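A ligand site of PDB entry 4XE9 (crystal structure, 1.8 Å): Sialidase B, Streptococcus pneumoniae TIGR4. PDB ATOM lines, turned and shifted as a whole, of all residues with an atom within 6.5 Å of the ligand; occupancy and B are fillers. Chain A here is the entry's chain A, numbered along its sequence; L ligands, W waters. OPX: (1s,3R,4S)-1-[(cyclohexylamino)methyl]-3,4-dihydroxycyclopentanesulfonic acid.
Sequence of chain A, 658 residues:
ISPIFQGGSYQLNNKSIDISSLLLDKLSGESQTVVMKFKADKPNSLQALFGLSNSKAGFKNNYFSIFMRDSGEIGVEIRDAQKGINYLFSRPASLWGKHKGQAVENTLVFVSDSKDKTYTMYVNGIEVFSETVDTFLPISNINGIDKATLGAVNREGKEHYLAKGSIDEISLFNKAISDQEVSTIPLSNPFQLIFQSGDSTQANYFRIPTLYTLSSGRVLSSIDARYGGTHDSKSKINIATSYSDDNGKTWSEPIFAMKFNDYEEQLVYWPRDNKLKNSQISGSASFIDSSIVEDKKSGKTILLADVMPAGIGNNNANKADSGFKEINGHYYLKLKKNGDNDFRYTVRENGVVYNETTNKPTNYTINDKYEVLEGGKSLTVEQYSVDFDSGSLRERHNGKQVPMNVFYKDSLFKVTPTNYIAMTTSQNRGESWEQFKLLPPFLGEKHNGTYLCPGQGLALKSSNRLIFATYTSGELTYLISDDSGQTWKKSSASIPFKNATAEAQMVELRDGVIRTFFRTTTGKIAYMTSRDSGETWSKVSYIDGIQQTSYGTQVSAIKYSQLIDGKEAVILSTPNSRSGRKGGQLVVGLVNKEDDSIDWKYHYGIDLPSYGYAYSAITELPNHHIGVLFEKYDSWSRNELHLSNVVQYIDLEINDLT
The side-chain amide oxygen (OE1) of Gln 456 sits at hydrogen-bond distance from an oxygen (OAC) of the ligand, at 2.8 Å. OAD of the ligand is in hydrogen-bond range of N of Thr 213, 3.0 Å away. OAE of the ligand is in salt-bridge range of NZ of Lys 461, at 3.0 Å. OAD of the ligand is in hydrogen-bond range of OG1 of Thr 619 (3.0 Å).
NE2 of Gln 456 sits at hydrogen-bond distance from O of Ile 618, 3.3 Å away. The side-chain amide nitrogen (NE2) of Gln 456 lies within hydrogen-bond range of the backbone carbonyl oxygen (O) of Leu 211, 2.7 Å away. The side-chain hydroxyl (OG1) of Thr 213 lies within hydrogen-bond range of the side-chain hydroxyl (OG1) of Thr 619 (2.7 Å). The backbone carbonyl oxygen (O) of Glu 620 sits at hydrogen-bond distance from the side-chain hydroxyl (OG1) of Thr 213, 2.7 Å away. The backbone NH (N) of Lys 461 sits at hydrogen-bond distance from the side-chain carboxylate (OE1) of Glu 508 (2.9 Å). The side-chain carboxylate of Glu 620 sits at hydrogen-bond distance from a ring nitrogen (ND1) of His 624, at 2.7 Å. The side-chain carboxylate (OE2) of Glu 620 sits at hydrogen-bond distance from the side-chain hydroxyl (OG) of Ser 561 (2.4 Å). OH of Tyr 212 sits at hydrogen-bond distance from N of Glu 294, 3.3 Å away.
Residues that only touch the ligand: Glu 620 (3.3 Å), Tyr 212 (3.5 Å), Ile 558 (3.7 Å), Leu 621 (3.7 Å) and Pro 622 (3.99 Å). Hydrophobic or aromatic side chains within 4 Å of the ligand: Tyr 212 and Ile 558. Within 4 Å of the ligand: Tyr 212, Thr 213, Gln 456, Lys 461, Ile 558, Thr 619, Glu 620, Leu 621 and Pro 622. The nearest printed residue that does not touch the ligand is Ala 459 (4.2 Å).
Water W7 lies within hydrogen-bond range of an oxygen (OAB) of the ligand, the side-chain hydroxyl (OH) of Tyr 212 and the backbone NH (N) of Ala 459. Water W5 bridges OH of Tyr 212 (2.7 Å) and OAA of the ligand (2.7 Å). Water W4 lies within hydrogen-bond range of the backbone NH of Glu 620 and an oxygen (OAC) of the ligand. Water W2 lies within hydrogen-bond range of the side-chain amino group of Lys 461 (2.9 Å), an oxygen (OAE) of the ligand (3.1 Å) and the backbone carbonyl oxygen of Lys 559 (3.2 Å). Water W3 bridges N of Lys 559 (2.9 Å) and OAC of the ligand (3.1 Å).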
ATOM      1  N   LEU A 211       7.958   2.188 -28.806  1.00  0.00           N
ATOM      2  CA  LEU A 211       6.546   1.928 -28.534  1.00  0.00           C
ATOM      3  C   LEU A 211       5.780   3.228 -28.685  1.00  0.00           C
ATOM      4  O   LEU A 211       6.287   4.290 -28.302  1.00  0.00           O
ATOM      5  CB  LEU A 211       6.335   1.427 -27.099  1.00  0.00           C
ATOM      6  CG  LEU A 211       6.675  -0.026 -26.741  1.00  0.00           C
ATOM      7  CD1 LEU A 211       6.593  -0.232 -25.223  1.00  0.00           C
ATOM      8  CD2 LEU A 211       5.722  -0.966 -27.469  1.00  0.00           C
ATOM      9  N   TYR A 212       4.567   3.152 -29.194  1.00  0.00           N
ATOM     10  CA  TYR A 212       3.754   4.346 -29.361  1.00  0.00           C
ATOM     11  C   TYR A 212       2.285   3.949 -29.339  1.00  0.00           C
ATOM     12  O   TYR A 212       1.885   2.974 -29.999  1.00  0.00           O
ATOM     13  CB  TYR A 212       4.131   5.036 -30.686  1.00  0.00           C
ATOM     14  CG  TYR A 212       3.606   6.449 -30.827  1.00  0.00           C
ATOM     15  CD1 TYR A 212       2.293   6.678 -31.172  1.00  0.00           C
ATOM     16  CD2 TYR A 212       4.448   7.536 -30.634  1.00  0.00           C
ATOM     17  CE1 TYR A 212       1.802   7.973 -31.314  1.00  0.00           C
ATOM     18  CE2 TYR A 212       3.965   8.842 -30.776  1.00  0.00           C
ATOM     19  CZ  TYR A 212       2.644   9.050 -31.120  1.00  0.00           C
ATOM     20  OH  TYR A 212       2.143  10.344 -31.264  1.00  0.00           O
ATOM     21  N   THR A 213       1.491   4.682 -28.566  1.00  0.00           N
ATOM     22  CA  THR A 213       0.061   4.369 -28.465  1.00  0.00           C
ATOM     23  C   THR A 213      -0.773   5.198 -29.454  1.00  0.00           C
ATOM     24  O   THR A 213      -0.759   6.419 -29.399  1.00  0.00           O
ATOM     25  CB  THR A 213      -0.450   4.582 -27.026  1.00  0.00           C
ATOM     26  OG1 THR A 213       0.386   3.855 -26.118  1.00  0.00           O
ATOM     27  CG2 THR A 213      -1.898   4.089 -26.888  1.00  0.00           C
ATOM     28  N   LEU A 214      -1.481   4.511 -30.351  1.00  0.00           N
ATOM     29  CA  LEU A 214      -2.246   5.176 -31.403  1.00  0.00           C
ATOM     30  C   LEU A 214      -3.647   5.539 -30.920  1.00  0.00           C
ATOM     31  O   LEU A 214      -4.143   4.959 -29.934  1.00  0.00           O
ATOM     32  CB  LEU A 214      -2.317   4.300 -32.648  1.00  0.00           C
ATOM     33  CG  LEU A 214      -0.974   3.794 -33.187  1.00  0.00           C
ATOM     34  CD1 LEU A 214      -1.192   2.843 -34.358  1.00  0.00           C
ATOM     35  CD2 LEU A 214      -0.091   4.970 -33.619  1.00  0.00           C
ATOM     36  N   GLU A 294       2.210   9.682 -34.499  1.00  0.00           N
ATOM     37  CA  GLU A 294       0.934   9.618 -35.194  1.00  0.00           C
ATOM     38  C   GLU A 294       0.425  11.025 -35.484  1.00  0.00           C
ATOM     39  O   GLU A 294       0.475  11.895 -34.609  1.00  0.00           O
ATOM     40  CB  GLU A 294      -0.117   8.824 -34.414  1.00  0.00           C
ATOM     41  CG  GLU A 294      -1.432   8.677 -35.188  1.00  0.00           C
ATOM     42  CD  GLU A 294      -2.435   7.783 -34.512  1.00  0.00           C
ATOM     43  OE1 GLU A 294      -2.827   8.091 -33.368  1.00  0.00           O
ATOM     44  OE2 GLU A 294      -2.839   6.773 -35.127  1.00  0.00           O
ATOM     45  N   LYS A 296      -2.616  13.514 -36.137  1.00  0.00           N
ATOM     46  CA  LYS A 296      -4.068  13.599 -35.909  1.00  0.00           C
ATOM     47  C   LYS A 296      -4.826  13.999 -37.146  1.00  0.00           C
ATOM     48  O   LYS A 296      -5.900  13.445 -37.447  1.00  0.00           O
ATOM     49  CB  LYS A 296      -4.386  14.616 -34.808  1.00  0.00           C
ATOM     50  CG  LYS A 296      -4.149  14.142 -33.389  1.00  0.00           C
ATOM     51  CD  LYS A 296      -4.328  15.307 -32.422  1.00  0.00           C
ATOM     52  CE  LYS A 296      -3.960  14.927 -30.991  1.00  0.00           C
ATOM     53  NZ  LYS A 296      -2.490  14.684 -30.790  1.00  0.00           N
ATOM     54  N   GLN A 456      10.055   7.856 -29.743  1.00  0.00           N
ATOM     55  CA  GLN A 456       8.853   8.511 -30.237  1.00  0.00           C
ATOM     56  C   GLN A 456       9.160   9.898 -30.771  1.00  0.00           C
ATOM     57  O   GLN A 456      10.032  10.601 -30.266  1.00  0.00           O
ATOM     58  CB  GLN A 456       7.838   8.663 -29.103  1.00  0.00           C
ATOM     59  CG  GLN A 456       7.514   7.393 -28.349  1.00  0.00           C
ATOM     60  CD  GLN A 456       6.460   7.606 -27.270  1.00  0.00           C
ATOM     61  OE1 GLN A 456       6.172   8.742 -26.870  1.00  0.00           O
ATOM     62  NE2 GLN A 456       5.869   6.509 -26.806  1.00  0.00           N
ATOM     63  N   GLY A 457       8.409  10.294 -31.801  1.00  0.00           N
ATOM     64  CA  GLY A 457       8.316  11.690 -32.141  1.00  0.00           C
ATOM     65  C   GLY A 457       7.225  12.251 -31.247  1.00  0.00           C
ATOM     66  O   GLY A 457       6.615  11.507 -30.457  1.00  0.00           O
ATOM     67  N   LEU A 458       6.946  13.536 -31.373  1.00  0.00           N
ATOM     68  CA  LEU A 458       5.973  14.185 -30.509  1.00  0.00           C
ATOM     69  C   LEU A 458       4.886  14.849 -31.341  1.00  0.00           C
ATOM     70  O   LEU A 458       5.181  15.645 -32.232  1.00  0.00           O
ATOM     71  CB  LEU A 458       6.653  15.233 -29.615  1.00  0.00           C
ATOM     72  CG  LEU A 458       5.676  16.096 -28.806  1.00  0.00           C
ATOM     73  CD1 LEU A 458       5.023  15.275 -27.699  1.00  0.00           C
ATOM     74  CD2 LEU A 458       6.389  17.330 -28.232  1.00  0.00           C
ATOM     75  N   ALA A 459       3.643  14.469 -31.088  1.00  0.00           N
ATOM     76  CA  ALA A 459       2.497  15.136 -31.685  1.00  0.00           C
ATOM     77  C   ALA A 459       1.921  16.056 -30.619  1.00  0.00           C
ATOM     78  O   ALA A 459       1.474  15.599 -29.576  1.00  0.00           O
ATOM     79  CB  ALA A 459       1.446  14.121 -32.137  1.00  0.00           C
ATOM     80  N   LEU A 460       1.976  17.355 -30.871  1.00  0.00           N
ATOM     81  CA  LEU A 460       1.473  18.319 -29.908  1.00  0.00           C
ATOM     82  C   LEU A 460      -0.049  18.200 -29.803  1.00  0.00           C
ATOM     83  O   LEU A 460      -0.731  18.008 -30.810  1.00  0.00           O
ATOM     84  CB  LEU A 460       1.887  19.732 -30.304  1.00  0.00           C
ATOM     85  CG  LEU A 460       3.348  20.040 -29.971  1.00  0.00           C
ATOM     86  CD1 LEU A 460       4.307  19.361 -30.915  1.00  0.00           C
ATOM     87  CD2 LEU A 460       3.552  21.504 -30.051  1.00  0.00           C
ATOM     88  N   LYS A 461      -0.565  18.314 -28.589  1.00  0.00           N
ATOM     89  CA  LYS A 461      -1.974  18.043 -28.325  1.00  0.00           C
ATOM     90  C   LYS A 461      -2.928  19.118 -28.862  1.00  0.00           C
ATOM     91  O   LYS A 461      -4.047  18.798 -29.287  1.00  0.00           O
ATOM     92  CB  LYS A 461      -2.201  17.801 -26.838  1.00  0.00           C
ATOM     93  CG  LYS A 461      -1.732  16.421 -26.374  1.00  0.00           C
ATOM     94  CD  LYS A 461      -2.146  16.106 -24.942  1.00  0.00           C
ATOM     95  CE  LYS A 461      -1.622  14.746 -24.522  1.00  0.00           C
ATOM     96  NZ  LYS A 461      -0.144  14.677 -24.727  1.00  0.00           N
ATOM     97  N   GLU A 508       5.202  16.585 -23.643  1.00  0.00           N
ATOM     98  CA  GLU A 508       4.511  17.871 -23.555  1.00  0.00           C
ATOM     99  C   GLU A 508       3.968  18.028 -22.135  1.00  0.00           C
ATOM    100  O   GLU A 508       3.062  17.311 -21.736  1.00  0.00           O
ATOM    101  CB  GLU A 508       3.388  17.969 -24.608  1.00  0.00           C
ATOM    102  CG  GLU A 508       2.783  19.367 -24.740  1.00  0.00           C
ATOM    103  CD  GLU A 508       1.809  19.493 -25.913  1.00  0.00           C
ATOM    104  OE1 GLU A 508       1.254  18.463 -26.339  1.00  0.00           O
ATOM    105  OE2 GLU A 508       1.615  20.630 -26.406  1.00  0.00           O
ATOM    106  N   ALA A 557      10.785   8.557 -22.291  1.00  0.00           N
ATOM    107  CA  ALA A 557      10.068   9.471 -21.422  1.00  0.00           C
ATOM    108  C   ALA A 557       8.650   9.672 -21.915  1.00  0.00           C
ATOM    109  O   ALA A 557       8.418   9.841 -23.106  1.00  0.00           O
ATOM    110  CB  ALA A 557      10.785  10.802 -21.378  1.00  0.00           C
ATOM    111  N   ILE A 558       7.688   9.651 -20.998  1.00  0.00           N
ATOM    112  CA  ILE A 558       6.318   9.963 -21.362  1.00  0.00           C
ATOM    113  C   ILE A 558       5.689  10.910 -20.368  1.00  0.00           C
ATOM    114  O   ILE A 558       6.142  11.029 -19.220  1.00  0.00           O
ATOM    115  CB  ILE A 558       5.449   8.703 -21.459  1.00  0.00           C
ATOM    116  CG1 ILE A 558       5.481   7.926 -20.146  1.00  0.00           C
ATOM    117  CG2 ILE A 558       5.886   7.839 -22.638  1.00  0.00           C
ATOM    118  CD1 ILE A 558       4.353   6.925 -20.010  1.00  0.00           C
ATOM    119  N   LYS A 559       4.631  11.593 -20.819  1.00  0.00           N
ATOM    120  CA  LYS A 559       3.773  12.356 -19.928  1.00  0.00           C
ATOM    121  C   LYS A 559       2.561  11.474 -19.667  1.00  0.00           C
ATOM    122  O   LYS A 559       1.846  11.115 -20.610  1.00  0.00           O
ATOM    123  CB  LYS A 559       3.330  13.649 -20.613  1.00  0.00           C
ATOM    124  CG  LYS A 559       2.236  14.401 -19.894  1.00  0.00           C
ATOM    125  CD  LYS A 559       2.778  15.056 -18.645  1.00  0.00           C
ATOM    126  CE  LYS A 559       1.663  15.779 -17.896  1.00  0.00           C
ATOM    127  NZ  LYS A 559       0.973  16.742 -18.793  1.00  0.00           N
ATOM    128  N   SER A 561      -1.177  10.288 -18.455  1.00  0.00           N
ATOM    129  CA  SER A 561      -2.439  11.001 -18.680  1.00  0.00           C
ATOM    130  C   SER A 561      -3.180  11.288 -17.380  1.00  0.00           C
ATOM    131  O   SER A 561      -4.009  12.204 -17.326  1.00  0.00           O
ATOM    132  CB  SER A 561      -3.341  10.220 -19.641  1.00  0.00           C
ATOM    133  OG  SER A 561      -3.856   9.047 -19.023  1.00  0.00           O
ATOM    134  N   ILE A 618       8.928   3.204 -23.663  1.00  0.00           N
ATOM    135  CA  ILE A 618       7.826   3.223 -22.724  1.00  0.00           C
ATOM    136  C   ILE A 618       6.602   3.892 -23.336  1.00  0.00           C
ATOM    137  O   ILE A 618       6.718   4.875 -24.064  1.00  0.00           O
ATOM    138  CB  ILE A 618       8.208   3.924 -21.396  1.00  0.00           C
ATOM    139  CG1 ILE A 618       7.030   3.941 -20.429  1.00  0.00           C
ATOM    140  CG2 ILE A 618       8.723   5.331 -21.661  1.00  0.00           C
ATOM    141  CD1 ILE A 618       7.373   4.480 -19.070  1.00  0.00           C
ATOM    142  N   THR A 619       5.426   3.337 -23.073  1.00  0.00           N
ATOM    143  CA  THR A 619       4.221   4.029 -23.510  1.00  0.00           C
ATOM    144  C   THR A 619       3.100   3.770 -22.524  1.00  0.00           C
ATOM    145  O   THR A 619       3.065   2.724 -21.877  1.00  0.00           O
ATOM    146  CB  THR A 619       3.804   3.646 -24.950  1.00  0.00           C
ATOM    147  OG1 THR A 619       2.938   4.658 -25.485  1.00  0.00           O
ATOM    148  CG2 THR A 619       3.084   2.307 -24.972  1.00  0.00           C
ATOM    149  N   GLU A 620       2.193   4.738 -22.398  1.00  0.00           N
ATOM    150  CA  GLU A 620       0.991   4.507 -21.622  1.00  0.00           C
ATOM    151  C   GLU A 620       0.016   3.737 -22.516  1.00  0.00           C
ATOM    152  O   GLU A 620      -0.378   4.208 -23.595  1.00  0.00           O
ATOM    153  CB  GLU A 620       0.375   5.836 -21.147  1.00  0.00           C
ATOM    154  CG  GLU A 620      -0.876   5.652 -20.284  1.00  0.00           C
ATOM    155  CD  GLU A 620      -1.476   6.969 -19.836  1.00  0.00           C
ATOM    156  OE1 GLU A 620      -0.823   8.023 -20.029  1.00  0.00           O
ATOM    157  OE2 GLU A 620      -2.611   6.966 -19.308  1.00  0.00           O
ATOM    158  N   LEU A 621      -0.357   2.546 -22.076  1.00  0.00           N
ATOM    159  CA  LEU A 621      -1.325   1.736 -22.800  1.00  0.00           C
ATOM    160  C   LEU A 621      -2.692   2.367 -22.636  1.00  0.00           C
ATOM    161  O   LEU A 621      -2.916   3.129 -21.695  1.00  0.00           O
ATOM    162  CB  LEU A 621      -1.310   0.306 -22.267  1.00  0.00           C
ATOM    163  CG  LEU A 621       0.094  -0.302 -22.365  1.00  0.00           C
ATOM    164  CD1 LEU A 621       0.186  -1.604 -21.577  1.00  0.00           C
ATOM    165  CD2 LEU A 621       0.467  -0.547 -23.805  1.00  0.00           C
ATOM    166  N   PRO A 622      -3.622   2.092 -23.565  1.00  0.00           N
ATOM    167  CA  PRO A 622      -4.941   2.732 -23.516  1.00  0.00           C
ATOM    168  C   PRO A 622      -5.675   2.537 -22.194  1.00  0.00           C
ATOM    169  O   PRO A 622      -6.507   3.390 -21.828  1.00  0.00           O
ATOM    170  CB  PRO A 622      -5.702   2.043 -24.646  1.00  0.00           C
ATOM    171  CG  PRO A 622      -4.617   1.720 -25.658  1.00  0.00           C
ATOM    172  CD  PRO A 622      -3.389   1.379 -24.846  1.00  0.00           C
ATOM    173  N   ASN A 623      -5.390   1.455 -21.487  1.00  0.00           N
ATOM    174  CA  ASN A 623      -6.042   1.149 -20.221  1.00  0.00           C
ATOM    175  C   ASN A 623      -5.310   1.741 -19.034  1.00  0.00           C
ATOM    176  O   ASN A 623      -5.570   1.384 -17.888  1.00  0.00           O
ATOM    177  CB  ASN A 623      -6.156  -0.374 -20.026  1.00  0.00           C
ATOM    178  CG  ASN A 623      -4.801  -1.056 -20.024  1.00  0.00           C
ATOM    179  OD1 ASN A 623      -3.775  -0.400 -20.181  1.00  0.00           O
ATOM    180  ND2 ASN A 623      -4.794  -2.376 -19.830  1.00  0.00           N
ATOM    181  N   HIS A 624      -4.345   2.617 -19.338  1.00  0.00           N
ATOM    182  CA  HIS A 624      -3.546   3.363 -18.350  1.00  0.00           C
ATOM    183  C   HIS A 624      -2.486   2.541 -17.628  1.00  0.00           C
ATOM    184  O   HIS A 624      -1.875   3.023 -16.685  1.00  0.00           O
ATOM    185  CB  HIS A 624      -4.441   4.125 -17.352  1.00  0.00           C
ATOM    186  CG  HIS A 624      -5.449   5.020 -18.001  1.00  0.00           C
ATOM    187  ND1 HIS A 624      -5.105   6.049 -18.848  1.00  0.00           N
ATOM    188  CD2 HIS A 624      -6.812   5.020 -17.953  1.00  0.00           C
ATOM    189  CE1 HIS A 624      -6.202   6.661 -19.268  1.00  0.00           C
ATOM    190  NE2 HIS A 624      -7.249   6.047 -18.751  1.00  0.00           N
HETATM  191  CAF OPX L   1      -4.047   6.899 -22.899  1.00  0.00           C
HETATM  192  CAG OPX L   1      -4.692   8.039 -23.623  1.00  0.00           C
HETATM  193  CAH OPX L   1      -3.039   6.232 -23.774  1.00  0.00           C
HETATM  194  CAI OPX L   1      -3.676   9.026 -24.124  1.00  0.00           C
HETATM  195  CAJ OPX L   1      -2.017   7.196 -24.302  1.00  0.00           C
HETATM  196  CAK OPX L   1      -0.691   8.826 -26.379  1.00  0.00           C
HETATM  197  CAL OPX L   1       1.549   9.544 -25.648  1.00  0.00           C
HETATM  198  CAM OPX L   1       1.190   9.041 -27.933  1.00  0.00           C
HETATM  199  CAO OPX L   1       2.846   9.300 -26.325  1.00  0.00           C
HETATM  200  CAP OPX L   1       2.427   8.367 -27.461  1.00  0.00           C
HETATM  201  CAQ OPX L   1      -2.642   8.373 -24.986  1.00  0.00           C
HETATM  202  CAR OPX L   1       0.553   9.658 -26.742  1.00  0.00           C
HETATM  203  NAN OPX L   1      -1.581   9.363 -25.326  1.00  0.00           N
HETATM  204  OAA OPX L   1      -0.667  11.455 -28.300  1.00  0.00           O
HETATM  205  OAB OPX L   1       1.445  12.067 -27.345  1.00  0.00           O
HETATM  206  OAC OPX L   1       3.685   8.674 -25.499  1.00  0.00           O
HETATM  207  OAD OPX L   1       2.134   7.154 -26.994  1.00  0.00           O
HETATM  208  OAE OPX L   1      -0.512  11.929 -25.935  1.00  0.00           O
HETATM  209  SAS OPX L   1       0.177  11.351 -27.101  1.00  0.00           S
HETATM  210  O   HOH W   1      -3.173  11.417 -27.089  1.00  0.00           O
HETATM  211  O   HOH W   2       1.304  12.485 -23.495  1.00  0.00           O
HETATM  212  O   HOH W   3       4.056  11.196 -23.663  1.00  0.00           O
HETATM  213  O   HOH W   4       2.507   7.353 -23.154  1.00  0.00           O
HETATM  214  O   HOH W   5      -0.479  10.771 -30.889  1.00  0.00           O
HETATM  215  O   HOH W   6      -0.589  10.583 -23.079  1.00  0.00           O
HETATM  216  O   HOH W   7       3.168  12.108 -29.387  1.00  0.00           O
